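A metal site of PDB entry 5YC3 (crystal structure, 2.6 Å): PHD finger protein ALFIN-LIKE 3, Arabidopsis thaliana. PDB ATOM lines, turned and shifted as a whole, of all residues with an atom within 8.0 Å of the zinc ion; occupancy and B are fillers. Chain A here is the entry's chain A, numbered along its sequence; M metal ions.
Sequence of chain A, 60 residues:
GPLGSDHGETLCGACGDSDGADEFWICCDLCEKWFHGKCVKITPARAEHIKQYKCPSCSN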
ATOM      1  N   LEU A  11     -31.837   6.166  35.837  1.00  0.00           N
ATOM      2  CA  LEU A  11     -30.843   7.207  35.651  1.00  0.00           C
ATOM      3  C   LEU A  11     -29.515   6.646  35.174  1.00  0.00           C
ATOM      4  O   LEU A  11     -29.034   5.631  35.681  1.00  0.00           O
ATOM      5  CB  LEU A  11     -30.640   7.993  36.951  1.00  0.00           C
ATOM      6  CG  LEU A  11     -31.875   8.727  37.451  1.00  0.00           C
ATOM      7  CD1 LEU A  11     -31.529   9.548  38.681  1.00  0.00           C
ATOM      8  CD2 LEU A  11     -32.465   9.608  36.370  1.00  0.00           C
ATOM      9  N   CYS A  12     -28.925   7.311  34.183  1.00  0.00           N
ATOM     10  CA  CYS A  12     -27.621   6.928  33.664  1.00  0.00           C
ATOM     11  C   CYS A  12     -26.575   7.089  34.751  1.00  0.00           C
ATOM     12  O   CYS A  12     -26.548   8.104  35.440  1.00  0.00           O
ATOM     13  CB  CYS A  12     -27.266   7.772  32.444  1.00  0.00           C
ATOM     14  SG  CYS A  12     -25.635   7.418  31.766  1.00  0.00           S
ATOM     15  N   GLY A  13     -25.712   6.085  34.905  1.00  0.00           N
ATOM     16  CA  GLY A  13     -24.705   6.103  35.950  1.00  0.00           C
ATOM     17  C   GLY A  13     -23.571   7.076  35.679  1.00  0.00           C
ATOM     18  O   GLY A  13     -22.751   7.326  36.563  1.00  0.00           O
ATOM     19  N   ALA A  14     -23.539   7.622  34.467  1.00  0.00           N
ATOM     20  CA  ALA A  14     -22.486   8.555  34.069  1.00  0.00           C
ATOM     21  C   ALA A  14     -22.945  10.008  34.095  1.00  0.00           C
ATOM     22  O   ALA A  14     -22.363  10.836  34.794  1.00  0.00           O
ATOM     23  CB  ALA A  14     -21.968   8.190  32.687  1.00  0.00           C
ATOM     24  N   CYS A  15     -23.997  10.317  33.337  1.00  0.00           N
ATOM     25  CA  CYS A  15     -24.476  11.697  33.221  1.00  0.00           C
ATOM     26  C   CYS A  15     -25.606  11.998  34.208  1.00  0.00           C
ATOM     27  O   CYS A  15     -25.838  13.154  34.553  1.00  0.00           O
ATOM     28  CB  CYS A  15     -24.937  11.973  31.786  1.00  0.00           C
ATOM     29  SG  CYS A  15     -26.446  11.100  31.310  1.00  0.00           S
ATOM     30  N   GLY A  16     -26.308  10.958  34.638  1.00  0.00           N
ATOM     31  CA  GLY A  16     -27.338  11.120  35.652  1.00  0.00           C
ATOM     32  C   GLY A  16     -28.677  11.590  35.115  1.00  0.00           C
ATOM     33  O   GLY A  16     -29.555  11.978  35.891  1.00  0.00           O
ATOM     34  N   ASP A  17     -28.848  11.562  33.800  1.00  0.00           N
ATOM     35  CA  ASP A  17     -30.124  11.953  33.196  1.00  0.00           C
ATOM     36  C   ASP A  17     -31.083  10.773  33.037  1.00  0.00           C
ATOM     37  O   ASP A  17     -30.710   9.616  33.196  1.00  0.00           O
ATOM     38  CB  ASP A  17     -29.895  12.594  31.831  1.00  0.00           C
ATOM     39  CG  ASP A  17     -29.409  14.028  31.922  1.00  0.00           C
ATOM     40  OD1 ASP A  17     -29.429  14.596  33.048  1.00  0.00           O
ATOM     41  OD2 ASP A  17     -29.033  14.591  30.884  1.00  0.00           O
ATOM     42  N   SER A  18     -32.339  11.088  32.717  1.00  0.00           N
ATOM     43  CA  SER A  18     -33.357  10.072  32.521  1.00  0.00           C
ATOM     44  C   SER A  18     -33.262   9.479  31.123  1.00  0.00           C
ATOM     45  O   SER A  18     -32.451   9.917  30.307  1.00  0.00           O
ATOM     46  CB  SER A  18     -34.753  10.663  32.749  1.00  0.00           C
ATOM     47  OG  SER A  18     -34.751  11.580  33.832  1.00  0.00           O
ATOM     48  N   GLU A  23     -32.906   5.924  22.359  1.00  0.00           N
ATOM     49  CA  GLU A  23     -31.568   5.896  22.938  1.00  0.00           C
ATOM     50  C   GLU A  23     -31.104   4.465  23.162  1.00  0.00           C
ATOM     51  O   GLU A  23     -31.896   3.591  23.490  1.00  0.00           O
ATOM     52  CB  GLU A  23     -31.549   6.662  24.261  1.00  0.00           C
ATOM     53  CG  GLU A  23     -31.923   8.122  24.138  1.00  0.00           C
ATOM     54  CD  GLU A  23     -31.996   8.802  25.488  1.00  0.00           C
ATOM     55  OE1 GLU A  23     -31.913   8.086  26.517  1.00  0.00           O
ATOM     56  OE2 GLU A  23     -32.134  10.041  25.531  1.00  0.00           O
ATOM     57  N   PHE A  24     -29.815   4.235  22.984  1.00  0.00           N
ATOM     58  CA  PHE A  24     -29.246   2.922  23.273  1.00  0.00           C
ATOM     59  C   PHE A  24     -28.660   2.885  24.683  1.00  0.00           C
ATOM     60  O   PHE A  24     -27.848   3.738  25.046  1.00  0.00           O
ATOM     61  CB  PHE A  24     -28.170   2.544  22.251  1.00  0.00           C
ATOM     62  CG  PHE A  24     -27.540   1.204  22.517  1.00  0.00           C
ATOM     63  CD1 PHE A  24     -28.231   0.035  22.256  1.00  0.00           C
ATOM     64  CD2 PHE A  24     -26.263   1.116  23.036  1.00  0.00           C
ATOM     65  CE1 PHE A  24     -27.661  -1.204  22.501  1.00  0.00           C
ATOM     66  CE2 PHE A  24     -25.673  -0.118  23.294  1.00  0.00           C
ATOM     67  CZ  PHE A  24     -26.380  -1.268  23.020  1.00  0.00           C
ATOM     68  N   TRP A  25     -29.081   1.896  25.456  1.00  0.00           N
ATOM     69  CA  TRP A  25     -28.623   1.750  26.828  1.00  0.00           C
ATOM     70  C   TRP A  25     -27.953   0.397  27.044  1.00  0.00           C
ATOM     71  O   TRP A  25     -28.234  -0.575  26.339  1.00  0.00           O
ATOM     72  CB  TRP A  25     -29.792   1.896  27.800  1.00  0.00           C
ATOM     73  CG  TRP A  25     -30.323   3.280  27.959  1.00  0.00           C
ATOM     74  CD1 TRP A  25     -31.018   3.999  27.035  1.00  0.00           C
ATOM     75  CD2 TRP A  25     -30.237   4.099  29.131  1.00  0.00           C
ATOM     76  NE1 TRP A  25     -31.354   5.234  27.557  1.00  0.00           N
ATOM     77  CE2 TRP A  25     -30.888   5.314  28.843  1.00  0.00           C
ATOM     78  CE3 TRP A  25     -29.656   3.924  30.393  1.00  0.00           C
ATOM     79  CZ2 TRP A  25     -30.982   6.342  29.767  1.00  0.00           C
ATOM     80  CZ3 TRP A  25     -29.750   4.952  31.317  1.00  0.00           C
ATOM     81  CH2 TRP A  25     -30.411   6.148  30.998  1.00  0.00           C
ATOM     82  N   TRP A  34     -27.487   1.308  34.832  1.00  0.00           N
ATOM     83  CA  TRP A  34     -27.719   1.507  33.409  1.00  0.00           C
ATOM     84  C   TRP A  34     -26.930   2.700  32.905  1.00  0.00           C
ATOM     85  O   TRP A  34     -26.670   3.647  33.643  1.00  0.00           O
ATOM     86  CB  TRP A  34     -29.208   1.712  33.126  1.00  0.00           C
ATOM     87  CG  TRP A  34     -30.004   0.448  33.030  1.00  0.00           C
ATOM     88  CD1 TRP A  34     -30.774  -0.125  34.005  1.00  0.00           C
ATOM     89  CD2 TRP A  34     -30.125  -0.389  31.872  1.00  0.00           C
ATOM     90  NE1 TRP A  34     -31.363  -1.270  33.527  1.00  0.00           N
ATOM     91  CE2 TRP A  34     -30.983  -1.454  32.224  1.00  0.00           C
ATOM     92  CE3 TRP A  34     -29.600  -0.342  30.585  1.00  0.00           C
ATOM     93  CZ2 TRP A  34     -31.313  -2.469  31.335  1.00  0.00           C
ATOM     94  CZ3 TRP A  34     -29.930  -1.357  29.695  1.00  0.00           C
ATOM     95  CH2 TRP A  34     -30.778  -2.399  30.069  1.00  0.00           C
ATOM     96  N   PHE A  35     -26.560   2.651  31.629  1.00  0.00           N
ATOM     97  CA  PHE A  35     -25.772   3.714  31.013  1.00  0.00           C
ATOM     98  C   PHE A  35     -26.228   4.005  29.596  1.00  0.00           C
ATOM     99  O   PHE A  35     -26.488   3.074  28.821  1.00  0.00           O
ATOM    100  CB  PHE A  35     -24.285   3.352  30.997  1.00  0.00           C
ATOM    101  CG  PHE A  35     -23.677   3.136  32.361  1.00  0.00           C
ATOM    102  CD1 PHE A  35     -23.733   1.894  32.971  1.00  0.00           C
ATOM    103  CD2 PHE A  35     -23.044   4.175  33.023  1.00  0.00           C
ATOM    104  CE1 PHE A  35     -23.170   1.694  34.232  1.00  0.00           C
ATOM    105  CE2 PHE A  35     -22.482   3.983  34.266  1.00  0.00           C
ATOM    106  CZ  PHE A  35     -22.546   2.747  34.878  1.00  0.00           C
ATOM    107  N   HIS A  36     -26.333   5.284  29.242  1.00  0.00           N
ATOM    108  CA  HIS A  36     -26.408   5.661  27.833  1.00  0.00           C
ATOM    109  C   HIS A  36     -25.217   5.045  27.123  1.00  0.00           C
ATOM    110  O   HIS A  36     -24.087   5.137  27.611  1.00  0.00           O
ATOM    111  CB  HIS A  36     -26.372   7.189  27.646  1.00  0.00           C
ATOM    112  CG  HIS A  36     -27.621   7.897  28.079  1.00  0.00           C
ATOM    113  ND1 HIS A  36     -27.683   8.639  29.237  1.00  0.00           N
ATOM    114  CD2 HIS A  36     -28.839   8.007  27.493  1.00  0.00           C
ATOM    115  CE1 HIS A  36     -28.888   9.169  29.363  1.00  0.00           C
ATOM    116  NE2 HIS A  36     -29.607   8.795  28.316  1.00  0.00           N
ATOM    117  N   GLY A  37     -25.459   4.405  25.974  1.00  0.00           N
ATOM    118  CA  GLY A  37     -24.380   3.888  25.164  1.00  0.00           C
ATOM    119  C   GLY A  37     -23.432   5.006  24.771  1.00  0.00           C
ATOM    120  O   GLY A  37     -22.218   4.816  24.708  1.00  0.00           O
ATOM    121  N   LYS A  38     -24.002   6.178  24.519  1.00  0.00           N
ATOM    122  CA  LYS A  38     -23.241   7.361  24.152  1.00  0.00           C
ATOM    123  C   LYS A  38     -22.316   7.830  25.275  1.00  0.00           C
ATOM    124  O   LYS A  38     -21.287   8.453  25.024  1.00  0.00           O
ATOM    125  CB  LYS A  38     -24.169   8.502  23.752  1.00  0.00           C
ATOM    126  CG  LYS A  38     -24.991   8.265  22.503  1.00  0.00           C
ATOM    127  CD  LYS A  38     -24.126   8.311  21.251  1.00  0.00           C
ATOM    128  CE  LYS A  38     -24.988   8.181  19.994  1.00  0.00           C
ATOM    129  NZ  LYS A  38     -26.040   9.241  19.918  1.00  0.00           N
ATOM    130  N   CYS A  39     -22.704   7.538  26.509  1.00  0.00           N
ATOM    131  CA  CYS A  39     -21.946   8.010  27.665  1.00  0.00           C
ATOM    132  C   CYS A  39     -20.754   7.105  27.997  1.00  0.00           C
ATOM    133  O   CYS A  39     -19.728   7.578  28.456  1.00  0.00           O
ATOM    134  CB  CYS A  39     -22.857   8.143  28.886  1.00  0.00           C
ATOM    135  SG  CYS A  39     -24.001   9.544  28.785  1.00  0.00           S
ATOM    136  N   VAL A  40     -20.906   5.810  27.762  1.00  0.00           N
ATOM    137  CA  VAL A  40     -19.803   4.874  27.960  1.00  0.00           C
ATOM    138  C   VAL A  40     -19.165   4.496  26.628  1.00  0.00           C
ATOM    139  O   VAL A  40     -18.328   3.591  26.553  1.00  0.00           O
ATOM    140  CB  VAL A  40     -20.248   3.599  28.704  1.00  0.00           C
ATOM    141  CG1 VAL A  40     -20.544   3.919  30.166  1.00  0.00           C
ATOM    142  CG2 VAL A  40     -21.459   2.980  28.026  1.00  0.00           C
HETATM  143 ZN    ZN M   1     -25.864   9.114  30.163  1.00  0.00          ZN
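The side-chain sulfur (SG) of Cys 12 sits close to the backbone NH (N) of Ala 14 (3.4 Å).
NE2 of His 36 is in hydrogen-bond range of OE1 of Glu 23 (3.0 Å).
The backbone NH (N) of Cys 12 is in hydrogen-bond range of the backbone carbonyl oxygen (O) of Asp 17.
N of Asp 17 sits close to SG of Cys 15, at 3.5 Å.
Four residues have an atom within 4 Å of the zinc ion: Cys 12, Cys 15, His 36 and Cys 39.
The nearest printed residue that does not touch the zinc ion is Ala 14 (4.7 Å).
ND1 of His 36 binds the zinc ion, at 2.1 Å.
The zinc ion is bound by the side-chain sulfur (SG) of Cys 12 (2.3 Å).
The zinc ion is bound by SG of Cys 39 (2.4 Å).
The zinc ion is bound by SG of Cys 15 (2.4 Å).
The zinc ion has four donor atoms within binding distance.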
